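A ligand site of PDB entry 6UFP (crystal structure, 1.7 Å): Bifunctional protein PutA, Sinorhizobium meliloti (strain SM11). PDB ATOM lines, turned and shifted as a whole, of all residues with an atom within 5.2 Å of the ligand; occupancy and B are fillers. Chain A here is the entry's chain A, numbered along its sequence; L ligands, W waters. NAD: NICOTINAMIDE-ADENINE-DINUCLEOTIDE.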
ATOM      1  N   ILE A 705     -31.464 -24.943   0.547  1.00  0.00           N
ATOM      2  CA  ILE A 705     -30.759 -24.039   1.433  1.00  0.00           C
ATOM      3  C   ILE A 705     -29.331 -24.539   1.488  1.00  0.00           C
ATOM      4  O   ILE A 705     -29.089 -25.703   1.817  1.00  0.00           O
ATOM      5  CB  ILE A 705     -31.417 -23.983   2.817  1.00  0.00           C
ATOM      6  CG1 ILE A 705     -32.848 -23.473   2.664  1.00  0.00           C
ATOM      7  CG2 ILE A 705     -30.655 -23.080   3.734  1.00  0.00           C
ATOM      8  CD1 ILE A 705     -33.694 -23.555   3.935  1.00  0.00           C
ATOM      9  N   SER A 706     -28.397 -23.685   1.097  1.00  0.00           N
ATOM     10  CA  SER A 706     -27.016 -24.096   0.890  1.00  0.00           C
ATOM     11  C   SER A 706     -26.077 -23.309   1.798  1.00  0.00           C
ATOM     12  O   SER A 706     -26.397 -22.196   2.236  1.00  0.00           O
ATOM     13  CB  SER A 706     -26.615 -23.913  -0.574  1.00  0.00           C
ATOM     14  OG  SER A 706     -26.893 -22.585  -1.007  1.00  0.00           O
ATOM     15  N   PRO A 707     -24.891 -23.860   2.084  1.00  0.00           N
ATOM     16  CA  PRO A 707     -23.981 -23.221   3.033  1.00  0.00           C
ATOM     17  C   PRO A 707     -22.982 -22.313   2.330  1.00  0.00           C
ATOM     18  O   PRO A 707     -22.861 -22.304   1.095  1.00  0.00           O
ATOM     19  CB  PRO A 707     -23.273 -24.439   3.646  1.00  0.00           C
ATOM     20  CG  PRO A 707     -23.087 -25.332   2.456  1.00  0.00           C
ATOM     21  CD  PRO A 707     -24.358 -25.148   1.606  1.00  0.00           C
ATOM     22  N   TRP A 708     -22.252 -21.540   3.138  1.00  0.00           N
ATOM     23  CA  TRP A 708     -21.289 -20.596   2.563  1.00  0.00           C
ATOM     24  C   TRP A 708     -19.974 -21.265   2.179  1.00  0.00           C
ATOM     25  O   TRP A 708     -19.199 -20.682   1.425  1.00  0.00           O
ATOM     26  CB  TRP A 708     -21.040 -19.448   3.541  1.00  0.00           C
ATOM     27  CG  TRP A 708     -20.350 -19.924   4.745  1.00  0.00           C
ATOM     28  CD1 TRP A 708     -20.896 -20.271   5.946  1.00  0.00           C
ATOM     29  CD2 TRP A 708     -18.953 -20.191   4.860  1.00  0.00           C
ATOM     30  NE1 TRP A 708     -19.924 -20.719   6.793  1.00  0.00           N
ATOM     31  CE2 TRP A 708     -18.715 -20.677   6.139  1.00  0.00           C
ATOM     32  CE3 TRP A 708     -17.872 -20.032   3.982  1.00  0.00           C
ATOM     33  CZ2 TRP A 708     -17.450 -21.021   6.572  1.00  0.00           C
ATOM     34  CZ3 TRP A 708     -16.629 -20.376   4.408  1.00  0.00           C
ATOM     35  CH2 TRP A 708     -16.433 -20.864   5.692  1.00  0.00           C
ATOM     36  N   ASN A 709     -19.685 -22.460   2.698  1.00  0.00           N
ATOM     37  CA  ASN A 709     -18.322 -22.987   2.589  1.00  0.00           C
ATOM     38  C   ASN A 709     -18.061 -23.719   1.286  1.00  0.00           C
ATOM     39  O   ASN A 709     -16.895 -23.817   0.878  1.00  0.00           O
ATOM     40  CB  ASN A 709     -18.002 -23.899   3.785  1.00  0.00           C
ATOM     41  CG  ASN A 709     -18.756 -25.212   3.733  1.00  0.00           C
ATOM     42  OD1 ASN A 709     -19.948 -25.245   3.442  1.00  0.00           O
ATOM     43  ND2 ASN A 709     -18.043 -26.296   4.023  1.00  0.00           N
ATOM     44  N   PHE A 710     -19.094 -24.231   0.624  1.00  0.00           N
ATOM     45  CA  PHE A 710     -19.002 -24.660  -0.769  1.00  0.00           C
ATOM     46  C   PHE A 710     -20.092 -23.918  -1.526  1.00  0.00           C
ATOM     47  O   PHE A 710     -21.101 -24.509  -1.943  1.00  0.00           O
ATOM     48  CB  PHE A 710     -19.121 -26.167  -0.930  1.00  0.00           C
ATOM     49  CG  PHE A 710     -17.884 -26.889  -0.529  1.00  0.00           C
ATOM     50  CD1 PHE A 710     -16.853 -27.064  -1.432  1.00  0.00           C
ATOM     51  CD2 PHE A 710     -17.725 -27.345   0.771  1.00  0.00           C
ATOM     52  CE1 PHE A 710     -15.688 -27.704  -1.061  1.00  0.00           C
ATOM     53  CE2 PHE A 710     -16.567 -27.992   1.147  1.00  0.00           C
ATOM     54  CZ  PHE A 710     -15.548 -28.177   0.236  1.00  0.00           C
ATOM     55  N   ILE A 714     -22.084 -27.208  -3.566  1.00  0.00           N
ATOM     56  CA  ILE A 714     -23.238 -27.765  -2.870  1.00  0.00           C
ATOM     57  C   ILE A 714     -24.503 -27.046  -3.289  1.00  0.00           C
ATOM     58  O   ILE A 714     -25.574 -27.655  -3.430  1.00  0.00           O
ATOM     59  CB  ILE A 714     -23.017 -27.721  -1.349  1.00  0.00           C
ATOM     60  CG1 ILE A 714     -21.923 -28.717  -0.971  1.00  0.00           C
ATOM     61  CG2 ILE A 714     -24.333 -28.040  -0.589  1.00  0.00           C
ATOM     62  CD1 ILE A 714     -21.675 -28.789   0.515  1.00  0.00           C
ATOM     63  N   LYS A 732     -32.070 -20.729  -1.804  1.00  0.00           N
ATOM     64  CA  LYS A 732     -31.735 -19.764  -0.748  1.00  0.00           C
ATOM     65  C   LYS A 732     -30.253 -19.913  -0.425  1.00  0.00           C
ATOM     66  O   LYS A 732     -29.870 -20.805   0.349  1.00  0.00           O
ATOM     67  CB  LYS A 732     -32.589 -20.004   0.491  1.00  0.00           C
ATOM     68  CG  LYS A 732     -33.018 -18.730   1.215  1.00  0.00           C
ATOM     69  CD  LYS A 732     -31.830 -17.906   1.691  1.00  0.00           C
ATOM     70  CE  LYS A 732     -31.095 -18.610   2.819  1.00  0.00           C
ATOM     71  NZ  LYS A 732     -29.961 -17.781   3.318  1.00  0.00           N
ATOM     72  N   PRO A 733     -29.374 -19.086  -0.992  1.00  0.00           N
ATOM     73  CA  PRO A 733     -27.953 -19.211  -0.696  1.00  0.00           C
ATOM     74  C   PRO A 733     -27.605 -18.633   0.668  1.00  0.00           C
ATOM     75  O   PRO A 733     -28.322 -17.793   1.216  1.00  0.00           O
ATOM     76  CB  PRO A 733     -27.288 -18.390  -1.806  1.00  0.00           C
ATOM     77  CG  PRO A 733     -28.282 -17.314  -2.093  1.00  0.00           C
ATOM     78  CD  PRO A 733     -29.660 -17.993  -1.942  1.00  0.00           C
ATOM     79  N   ALA A 734     -26.477 -19.077   1.192  1.00  0.00           N
ATOM     80  CA  ALA A 734     -26.000 -18.530   2.448  1.00  0.00           C
ATOM     81  C   ALA A 734     -25.822 -17.018   2.330  1.00  0.00           C
ATOM     82  O   ALA A 734     -25.484 -16.475   1.267  1.00  0.00           O
ATOM     83  CB  ALA A 734     -24.684 -19.181   2.857  1.00  0.00           C
ATOM     84  N   GLU A 735     -26.064 -16.320   3.441  1.00  0.00           N
ATOM     85  CA  GLU A 735     -26.011 -14.858   3.412  1.00  0.00           C
ATOM     86  C   GLU A 735     -24.620 -14.350   3.047  1.00  0.00           C
ATOM     87  O   GLU A 735     -24.497 -13.292   2.417  1.00  0.00           O
ATOM     88  CB  GLU A 735     -26.456 -14.295   4.777  1.00  0.00           C
ATOM     89  CG  GLU A 735     -25.845 -14.982   5.998  1.00  0.00           C
ATOM     90  CD  GLU A 735     -26.645 -16.188   6.477  1.00  0.00           C
ATOM     91  OE1 GLU A 735     -26.940 -17.101   5.670  1.00  0.00           O
ATOM     92  OE2 GLU A 735     -26.982 -16.228   7.685  1.00  0.00           O
ATOM     93  N   GLU A 736     -23.576 -15.123   3.359  1.00  0.00           N
ATOM     94  CA  GLU A 736     -22.213 -14.657   3.116  1.00  0.00           C
ATOM     95  C   GLU A 736     -21.787 -14.762   1.659  1.00  0.00           C
ATOM     96  O   GLU A 736     -20.885 -14.021   1.244  1.00  0.00           O
ATOM     97  CB  GLU A 736     -21.240 -15.455   3.984  1.00  0.00           C
ATOM     98  CG  GLU A 736     -21.490 -15.300   5.481  1.00  0.00           C
ATOM     99  CD  GLU A 736     -22.427 -16.362   6.038  1.00  0.00           C
ATOM    100  OE1 GLU A 736     -22.452 -16.517   7.288  1.00  0.00           O
ATOM    101  OE2 GLU A 736     -23.133 -17.049   5.251  1.00  0.00           O
ATOM    102  N   GLY A 763     -30.587 -13.803   1.070  1.00  0.00           N
ATOM    103  CA  GLY A 763     -30.968 -13.287   2.370  1.00  0.00           C
ATOM    104  C   GLY A 763     -30.468 -14.205   3.476  1.00  0.00           C
ATOM    105  O   GLY A 763     -29.707 -15.135   3.248  1.00  0.00           O
ATOM    106  N   ASP A 764     -30.922 -13.901   4.695  1.00  0.00           N
ATOM    107  CA  ASP A 764     -30.505 -14.626   5.888  1.00  0.00           C
ATOM    108  C   ASP A 764     -31.463 -15.787   6.177  1.00  0.00           C
ATOM    109  O   ASP A 764     -32.288 -16.171   5.341  1.00  0.00           O
ATOM    110  CB  ASP A 764     -30.415 -13.672   7.077  1.00  0.00           C
ATOM    111  CG  ASP A 764     -31.659 -12.800   7.232  1.00  0.00           C
ATOM    112  OD1 ASP A 764     -32.776 -13.321   7.063  1.00  0.00           O
ATOM    113  OD2 ASP A 764     -31.496 -11.600   7.526  1.00  0.00           O
ATOM    114  N   GLY A 765     -31.361 -16.358   7.375  1.00  0.00           N
ATOM    115  CA  GLY A 765     -32.166 -17.505   7.735  1.00  0.00           C
ATOM    116  C   GLY A 765     -33.645 -17.215   7.820  1.00  0.00           C
ATOM    117  O   GLY A 765     -34.454 -18.145   7.700  1.00  0.00           O
ATOM    118  N   GLY A 768     -34.809 -18.189   4.637  1.00  0.00           N
ATOM    119  CA  GLY A 768     -34.880 -19.643   4.697  1.00  0.00           C
ATOM    120  C   GLY A 768     -36.105 -20.118   5.451  1.00  0.00           C
ATOM    121  O   GLY A 768     -36.812 -21.024   4.986  1.00  0.00           O
ATOM    122  N   ALA A 769     -36.395 -19.508   6.593  1.00  0.00           N
ATOM    123  CA  ALA A 769     -37.520 -19.958   7.406  1.00  0.00           C
ATOM    124  C   ALA A 769     -38.853 -19.660   6.714  1.00  0.00           C
ATOM    125  O   ALA A 769     -39.776 -20.477   6.766  1.00  0.00           O
ATOM    126  CB  ALA A 769     -37.474 -19.293   8.788  1.00  0.00           C
ATOM    127  N   VAL A 772     -39.304 -22.339   4.072  1.00  0.00           N
ATOM    128  CA  VAL A 772     -39.612 -23.640   4.665  1.00  0.00           C
ATOM    129  C   VAL A 772     -41.056 -23.688   5.130  1.00  0.00           C
ATOM    130  O   VAL A 772     -41.760 -24.687   4.949  1.00  0.00           O
ATOM    131  CB  VAL A 772     -38.630 -23.947   5.821  1.00  0.00           C
ATOM    132  CG1 VAL A 772     -39.029 -25.231   6.531  1.00  0.00           C
ATOM    133  CG2 VAL A 772     -37.210 -24.074   5.280  1.00  0.00           C
ATOM    134  N   PHE A 782     -31.243 -29.289   2.768  1.00  0.00           N
ATOM    135  CA  PHE A 782     -30.481 -28.408   3.634  1.00  0.00           C
ATOM    136  C   PHE A 782     -29.073 -28.953   3.816  1.00  0.00           C
ATOM    137  O   PHE A 782     -28.901 -30.144   4.081  1.00  0.00           O
ATOM    138  CB  PHE A 782     -31.151 -28.255   5.004  1.00  0.00           C
ATOM    139  CG  PHE A 782     -30.322 -27.480   5.967  1.00  0.00           C
ATOM    140  CD1 PHE A 782     -30.303 -26.096   5.935  1.00  0.00           C
ATOM    141  CD2 PHE A 782     -29.545 -28.131   6.923  1.00  0.00           C
ATOM    142  CE1 PHE A 782     -29.532 -25.365   6.825  1.00  0.00           C
ATOM    143  CE2 PHE A 782     -28.780 -27.406   7.817  1.00  0.00           C
ATOM    144  CZ  PHE A 782     -28.773 -26.032   7.778  1.00  0.00           C
ATOM    145  N   THR A 783     -28.096 -28.067   3.694  1.00  0.00           N
ATOM    146  CA  THR A 783     -26.720 -28.380   4.081  1.00  0.00           C
ATOM    147  C   THR A 783     -26.220 -27.260   4.968  1.00  0.00           C
ATOM    148  O   THR A 783     -26.229 -26.083   4.558  1.00  0.00           O
ATOM    149  CB  THR A 783     -25.820 -28.562   2.846  1.00  0.00           C
ATOM    150  OG1 THR A 783     -26.335 -29.632   2.050  1.00  0.00           O
ATOM    151  CG2 THR A 783     -24.424 -28.909   3.258  1.00  0.00           C
ATOM    152  N   GLY A 784     -25.799 -27.598   6.176  1.00  0.00           N
ATOM    153  CA  GLY A 784     -25.447 -26.589   7.163  1.00  0.00           C
ATOM    154  C   GLY A 784     -25.240 -27.222   8.524  1.00  0.00           C
ATOM    155  O   GLY A 784     -24.999 -28.423   8.631  1.00  0.00           O
ATOM    156  N   SER A 785     -25.341 -26.384   9.561  1.00  0.00           N
ATOM    157  CA  SER A 785     -25.143 -26.869  10.915  1.00  0.00           C
ATOM    158  C   SER A 785     -26.276 -27.799  11.371  1.00  0.00           C
ATOM    159  O   SER A 785     -27.413 -27.700  10.903  1.00  0.00           O
ATOM    160  CB  SER A 785     -25.020 -25.701  11.882  1.00  0.00           C
ATOM    161  OG  SER A 785     -26.172 -24.875  11.862  1.00  0.00           O
ATOM    162  N   THR A 786     -25.947 -28.687  12.314  1.00  0.00           N
ATOM    163  CA  THR A 786     -26.958 -29.569  12.886  1.00  0.00           C
ATOM    164  C   THR A 786     -28.050 -28.788  13.609  1.00  0.00           C
ATOM    165  O   THR A 786     -29.227 -29.158  13.545  1.00  0.00           O
ATOM    166  CB  THR A 786     -26.287 -30.568  13.832  1.00  0.00           C
ATOM    167  OG1 THR A 786     -25.303 -31.322  13.110  1.00  0.00           O
ATOM    168  CG2 THR A 786     -27.302 -31.516  14.440  1.00  0.00           C
ATOM    169  N   VAL A 788     -29.305 -25.802  12.971  1.00  0.00           N
ATOM    170  CA  VAL A 788     -30.267 -25.183  12.069  1.00  0.00           C
ATOM    171  C   VAL A 788     -31.125 -26.247  11.406  1.00  0.00           C
ATOM    172  O   VAL A 788     -32.339 -26.075  11.234  1.00  0.00           O
ATOM    173  CB  VAL A 788     -29.557 -24.294  11.047  1.00  0.00           C
ATOM    174  CG1 VAL A 788     -30.506 -23.913   9.926  1.00  0.00           C
ATOM    175  CG2 VAL A 788     -29.042 -23.017  11.736  1.00  0.00           C
ATOM    176  N   LEU A 791     -33.829 -26.984  13.655  1.00  0.00           N
ATOM    177  CA  LEU A 791     -34.905 -25.994  13.593  1.00  0.00           C
ATOM    178  C   LEU A 791     -35.808 -26.216  12.383  1.00  0.00           C
ATOM    179  O   LEU A 791     -37.022 -26.011  12.468  1.00  0.00           O
ATOM    180  CB  LEU A 791     -34.311 -24.586  13.562  1.00  0.00           C
ATOM    181  CG  LEU A 791     -33.728 -24.044  14.867  1.00  0.00           C
ATOM    182  CD1 LEU A 791     -32.899 -22.819  14.579  1.00  0.00           C
ATOM    183  CD2 LEU A 791     -34.858 -23.730  15.848  1.00  0.00           C
ATOM    184  N   ILE A 792     -35.229 -26.621  11.257  1.00  0.00           N
ATOM    185  CA  ILE A 792     -36.026 -26.872  10.063  1.00  0.00           C
ATOM    186  C   ILE A 792     -36.898 -28.105  10.261  1.00  0.00           C
ATOM    187  O   ILE A 792     -38.097 -28.102   9.946  1.00  0.00           O
ATOM    188  CB  ILE A 792     -35.121 -27.011   8.830  1.00  0.00           C
ATOM    189  CG1 ILE A 792     -34.505 -25.654   8.481  1.00  0.00           C
ATOM    190  CG2 ILE A 792     -35.881 -27.606   7.646  1.00  0.00           C
ATOM    191  CD1 ILE A 792     -33.322 -25.751   7.542  1.00  0.00           C
ATOM    192  N   GLU A 812     -27.793 -32.499   5.459  1.00  0.00           N
ATOM    193  CA  GLU A 812     -26.400 -32.925   5.589  1.00  0.00           C
ATOM    194  C   GLU A 812     -25.688 -31.921   6.491  1.00  0.00           C
ATOM    195  O   GLU A 812     -25.618 -30.733   6.179  1.00  0.00           O
ATOM    196  CB  GLU A 812     -25.770 -33.055   4.198  1.00  0.00           C
ATOM    197  CG  GLU A 812     -26.621 -33.981   3.281  1.00  0.00           C
ATOM    198  CD  GLU A 812     -26.701 -35.443   3.766  1.00  0.00           C
ATOM    199  OE1 GLU A 812     -25.773 -36.220   3.473  1.00  0.00           O
ATOM    200  OE2 GLU A 812     -27.692 -35.839   4.445  1.00  0.00           O
ATOM    201  N   THR A 813     -25.202 -32.413   7.641  1.00  0.00           N
ATOM    202  CA  THR A 813     -24.795 -31.517   8.700  1.00  0.00           C
ATOM    203  C   THR A 813     -23.341 -31.762   9.112  1.00  0.00           C
ATOM    204  O   THR A 813     -22.566 -32.292   8.310  1.00  0.00           O
ATOM    205  CB  THR A 813     -25.765 -31.672   9.880  1.00  0.00           C
ATOM    206  OG1 THR A 813     -25.985 -33.060  10.151  1.00  0.00           O
ATOM    207  CG2 THR A 813     -27.113 -31.043   9.485  1.00  0.00           C
ATOM    208  N   GLY A 814     -22.964 -31.377  10.317  1.00  0.00           N
ATOM    209  CA  GLY A 814     -21.553 -31.336  10.674  1.00  0.00           C
ATOM    210  C   GLY A 814     -20.920 -32.706  10.898  1.00  0.00           C
ATOM    211  O   GLY A 814     -21.527 -33.766  10.762  1.00  0.00           O
ATOM    212  N   GLY A 815     -19.639 -32.667  11.252  1.00  0.00           N
ATOM    213  CA  GLY A 815     -18.930 -33.866  11.657  1.00  0.00           C
ATOM    214  C   GLY A 815     -17.841 -33.499  12.626  1.00  0.00           C
ATOM    215  O   GLY A 815     -17.333 -32.377  12.629  1.00  0.00           O
ATOM    216  N   CYS A 846     -16.883 -29.580   5.775  1.00  0.00           N
ATOM    217  CA  CYS A 846     -17.605 -30.481   6.661  1.00  0.00           C
ATOM    218  C   CYS A 846     -16.774 -31.717   6.964  1.00  0.00           C
ATOM    219  O   CYS A 846     -16.905 -32.313   8.036  1.00  0.00           O
ATOM    220  CB  CYS A 846     -18.919 -30.906   6.023  1.00  0.00           C
ATOM    221  SG  CYS A 846     -18.714 -31.667   4.416  1.00  0.00           S
ATOM    222  N   GLU A 942     -18.669 -29.307  17.283  1.00  0.00           N
ATOM    223  CA  GLU A 942     -17.796 -29.044  16.141  1.00  0.00           C
ATOM    224  C   GLU A 942     -17.292 -27.610  16.177  1.00  0.00           C
ATOM    225  O   GLU A 942     -18.044 -26.675  16.489  1.00  0.00           O
ATOM    226  CB  GLU A 942     -18.572 -29.329  14.843  1.00  0.00           C
ATOM    227  CG  GLU A 942     -17.875 -28.917  13.546  1.00  0.00           C
ATOM    228  CD  GLU A 942     -18.814 -28.940  12.344  1.00  0.00           C
ATOM    229  OE1 GLU A 942     -18.652 -29.800  11.462  1.00  0.00           O
ATOM    230  OE2 GLU A 942     -19.730 -28.085  12.288  1.00  0.00           O
ATOM    231  N   PHE A 944     -15.696 -25.059  13.674  1.00  0.00           N
ATOM    232  CA  PHE A 944     -15.612 -25.024  12.214  1.00  0.00           C
ATOM    233  C   PHE A 944     -14.510 -24.056  11.769  1.00  0.00           C
ATOM    234  O   PHE A 944     -14.745 -22.951  11.284  1.00  0.00           O
ATOM    235  CB  PHE A 944     -16.964 -24.632  11.624  1.00  0.00           C
ATOM    236  CG  PHE A 944     -17.155 -25.119  10.226  1.00  0.00           C
ATOM    237  CD1 PHE A 944     -17.261 -26.493   9.964  1.00  0.00           C
ATOM    238  CD2 PHE A 944     -17.245 -24.236   9.165  1.00  0.00           C
ATOM    239  CE1 PHE A 944     -17.436 -26.951   8.670  1.00  0.00           C
ATOM    240  CE2 PHE A 944     -17.428 -24.690   7.866  1.00  0.00           C
ATOM    241  CZ  PHE A 944     -17.522 -26.057   7.629  1.00  0.00           C
ATOM    242  N   LEU A 972     -19.397 -38.625   9.925  1.00  0.00           N
ATOM    243  CA  LEU A 972     -19.235 -38.127   8.569  1.00  0.00           C
ATOM    244  C   LEU A 972     -18.003 -38.740   7.917  1.00  0.00           C
ATOM    245  O   LEU A 972     -18.109 -39.758   7.238  1.00  0.00           O
ATOM    246  CB  LEU A 972     -19.161 -36.601   8.568  1.00  0.00           C
ATOM    247  CG  LEU A 972     -19.235 -35.913   7.202  1.00  0.00           C
ATOM    248  CD1 LEU A 972     -20.298 -36.568   6.329  1.00  0.00           C
ATOM    249  CD2 LEU A 972     -19.546 -34.431   7.401  1.00  0.00           C
ATOM    250  N   PHE A1012     -21.015 -38.829  -0.960  1.00  0.00           N
ATOM    251  CA  PHE A1012     -20.653 -38.143   0.269  1.00  0.00           C
ATOM    252  C   PHE A1012     -21.856 -37.943   1.172  1.00  0.00           C
ATOM    253  O   PHE A1012     -22.905 -37.449   0.734  1.00  0.00           O
ATOM    254  CB  PHE A1012     -20.013 -36.782  -0.019  1.00  0.00           C
ATOM    255  CG  PHE A1012     -19.513 -36.133   1.213  1.00  0.00           C
ATOM    256  CD1 PHE A1012     -18.289 -36.520   1.749  1.00  0.00           C
ATOM    257  CD2 PHE A1012     -20.260 -35.182   1.872  1.00  0.00           C
ATOM    258  CE1 PHE A1012     -17.819 -35.946   2.904  1.00  0.00           C
ATOM    259  CE2 PHE A1012     -19.784 -34.605   3.040  1.00  0.00           C
ATOM    260  CZ  PHE A1012     -18.568 -34.985   3.553  1.00  0.00           C
ATOM    261  N   SER A1018     -24.585 -36.351  11.656  1.00  0.00           N
ATOM    262  CA  SER A1018     -23.967 -35.830  10.444  1.00  0.00           C
ATOM    263  C   SER A1018     -24.902 -35.803   9.250  1.00  0.00           C
ATOM    264  O   SER A1018     -24.536 -35.230   8.221  1.00  0.00           O
ATOM    265  CB  SER A1018     -22.722 -36.643  10.071  1.00  0.00           C
ATOM    266  OG  SER A1018     -21.728 -36.482  11.062  1.00  0.00           O
HETATM  267  PA  NAD L   1     -25.537 -22.675   8.859  1.00  0.00           P
HETATM  268  O1A NAD L   1     -26.336 -23.746   9.564  1.00  0.00           O
HETATM  269  O2A NAD L   1     -25.212 -21.568   9.797  1.00  0.00           O
HETATM  270  O5B NAD L   1     -26.368 -22.055   7.557  1.00  0.00           O
HETATM  271  C5B NAD L   1     -26.676 -22.889   6.435  1.00  0.00           C
HETATM  272  C4B NAD L   1     -27.982 -22.305   5.735  1.00  0.00           C
HETATM  273  O4B NAD L   1     -29.011 -22.385   6.533  1.00  0.00           O
HETATM  274  C3B NAD L   1     -27.833 -20.800   5.399  1.00  0.00           C
HETATM  275  O3B NAD L   1     -28.247 -20.579   4.108  1.00  0.00           O
HETATM  276  C2B NAD L   1     -28.769 -20.078   6.397  1.00  0.00           C
HETATM  277  O2B NAD L   1     -29.234 -18.808   5.769  1.00  0.00           O
HETATM  278  C1B NAD L   1     -29.742 -20.924   6.537  1.00  0.00           C
HETATM  279  N9A NAD L   1     -30.471 -20.827   7.775  1.00  0.00           N
HETATM  280  C8A NAD L   1     -30.011 -20.422   8.967  1.00  0.00           C
HETATM  281  N7A NAD L   1     -31.014 -20.506   9.835  1.00  0.00           N
HETATM  282  C5A NAD L   1     -32.105 -20.959   9.199  1.00  0.00           C
HETATM  283  C6A NAD L   1     -33.395 -21.237   9.620  1.00  0.00           C
HETATM  284  N6A NAD L   1     -33.973 -21.101  10.961  1.00  0.00           N
HETATM  285  N1A NAD L   1     -34.297 -21.699   8.770  1.00  0.00           N
HETATM  286  C2A NAD L   1     -33.943 -21.893   7.485  1.00  0.00           C
HETATM  287  N3A NAD L   1     -32.686 -21.627   7.067  1.00  0.00           N
HETATM  288  C4A NAD L   1     -31.768 -21.171   7.928  1.00  0.00           C
HETATM  289  O3  NAD L   1     -24.138 -23.377   8.285  1.00  0.00           O
HETATM  290  PN  NAD L   1     -22.942 -22.607   7.442  1.00  0.00           P
HETATM  291  O1N NAD L   1     -22.372 -21.479   8.326  1.00  0.00           O
HETATM  292  O2N NAD L   1     -23.466 -22.032   6.141  1.00  0.00           O
HETATM  293  O5D NAD L   1     -21.760 -23.726   7.130  1.00  0.00           O
HETATM  294  C5D NAD L   1     -21.171 -24.374   8.205  1.00  0.00           C
HETATM  295  C4D NAD L   1     -21.885 -25.726   8.493  1.00  0.00           C
HETATM  296  O4D NAD L   1     -22.199 -26.363   7.372  1.00  0.00           O
HETATM  297  C3D NAD L   1     -20.921 -26.648   9.224  1.00  0.00           C
HETATM  298  O3D NAD L   1     -21.484 -27.108  10.359  1.00  0.00           O
HETATM  299  C2D NAD L   1     -20.669 -27.833   8.217  1.00  0.00           C
HETATM  300  O2D NAD L   1     -20.321 -29.090   8.944  1.00  0.00           O
HETATM  301  C1D NAD L   1     -21.794 -27.923   7.596  1.00  0.00           C
HETATM  302  N1N NAD L   1     -21.618 -28.599   6.300  1.00  0.00           N
HETATM  303  C2N NAD L   1     -22.021 -29.891   6.120  1.00  0.00           C
HETATM  304  C3N NAD L   1     -21.849 -30.498   4.870  1.00  0.00           C
HETATM  305  C7N NAD L   1     -22.263 -31.952   4.605  1.00  0.00           C
HETATM  306  O7N NAD L   1     -22.335 -32.327   3.474  1.00  0.00           O
HETATM  307  N7N NAD L   1     -22.546 -32.890   5.677  1.00  0.00           N
HETATM  308  C4N NAD L   1     -21.263 -29.771   3.848  1.00  0.00           C
HETATM  309  C5N NAD L   1     -20.862 -28.502   4.036  1.00  0.00           C
HETATM  310  C6N NAD L   1     -21.055 -27.902   5.273  1.00  0.00           C
HETATM  311  O   HOH W   1     -24.812 -19.196   6.354  1.00  0.00           O
HETATM  312  O   HOH W   2     -23.891 -35.703   5.706  1.00  0.00           O
HETATM  313  O   HOH W   3     -36.786 -22.878   9.919  1.00  0.00           O
HETATM  314  O   HOH W   4     -23.385 -33.234   1.064  1.00  0.00           O
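The backbone NH of Ser 785 sits at hydrogen-bond distance from an oxygen (O1A) of the ligand, at 2.8 Å.
An oxygen (O1A) of the ligand is in hydrogen-bond range of the side-chain hydroxyl (OG) of Ser 785, at 2.6 Å.
The backbone carbonyl oxygen (O) of Thr 813 is in hydrogen-bond range of a nitrogen (N7N) of the ligand (2.7 Å).
O2B of the ligand is in hydrogen-bond range of NZ of Lys 732, at 2.8 Å.
The side-chain carboxylate (OE2) of Glu 942 is in hydrogen-bond range of an oxygen (O3D) of the ligand (2.8 Å).
An oxygen (O2B) of the ligand is in hydrogen-bond range of the side-chain carboxylate (OE1) of Glu 735 (2.9 Å).
The backbone NH of Trp 708 lies close to an oxygen (O2N) of the ligand (3.3 Å).
An oxygen (O1N) of the ligand is in hydrogen-bond range of the indole nitrogen (NE1) of Trp 708 (3.0 Å).
An oxygen (O3B) of the ligand lies within hydrogen-bond range of the backbone carbonyl oxygen (O) of Ser 706.
SG of Cys 846 sits close to O7N of the ligand, 3.8 Å away.
The side-chain hydroxyl of Ser 785 lies close to the backbone NH of Val 788 (3.5 Å).
The side-chain hydroxyl (OG1) of Thr 813 sits close to the side-chain hydroxyl (OG1) of Thr 786 (3.5 Å).
The side-chain amino group of Lys 732 lies within salt-bridge range of the side-chain carboxylate of Glu 735, 3.9 Å away.
N of Ser 706 lies within hydrogen-bond range of O of Lys 732.
NZ of Lys 732 is in hydrogen-bond range of O of Gly 763 (2.7 Å).
O of Ser 706 sits at hydrogen-bond distance from N of Ala 734 (3.3 Å).
O of Gly 814 is in hydrogen-bond range of OG of Ser 1018, 2.7 Å away.
N of Thr 783 is in hydrogen-bond range of O of Ile 705 (3.2 Å).
CG2 of Ile 705 touches O4B of the ligand, at 3.3 Å.
Pro 707 touches the ligand.
Asn 709 touches the ligand (OD1 to C6N, 3.4 Å).
Ile 714 touches the ligand.
CA of Ala 734 touches O3B of the ligand, at 3.5 Å.
Asp 764 touches the ligand (C to O2B, 3.8 Å).
N of Gly 765 touches O2B of the ligand (3.6 Å).
C of Gly 768 touches C2A of the ligand, 3.5 Å away.
Ala 769 touches the ligand.
CE1 of Phe 782 touches O4B of the ligand (3.0 Å).
Thr 783 touches the ligand (CG2 to C4N, 3.3 Å).
Gly 784 touches the ligand (CA to O4D, 3.3 Å).
Val 788 touches the ligand.
Ile 792 touches the ligand (CD1 to C2A, 3.9 Å).
Glu 812 touches the ligand.
Gly 814 touches the ligand.
Phe 944 touches the ligand (CE1 to C2D, 3.4 Å).
CD2 of Leu 972 touches N7N of the ligand, at 3.8 Å.
Phe 1012 touches the ligand (CE2 to O7N, 3.4 Å).
O of Ser 1018 touches N7N of the ligand, 3.99 Å away.
Water W2 lies within hydrogen-bond range of O of Ser 1018, OE1 of Glu 812 and N7N of the ligand.
Water W1 lies within hydrogen-bond range of OE2 of Glu 736 (2.9 Å), OE1 of Glu 735 (3.1 Å) and O2N of the ligand (3.1 Å).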
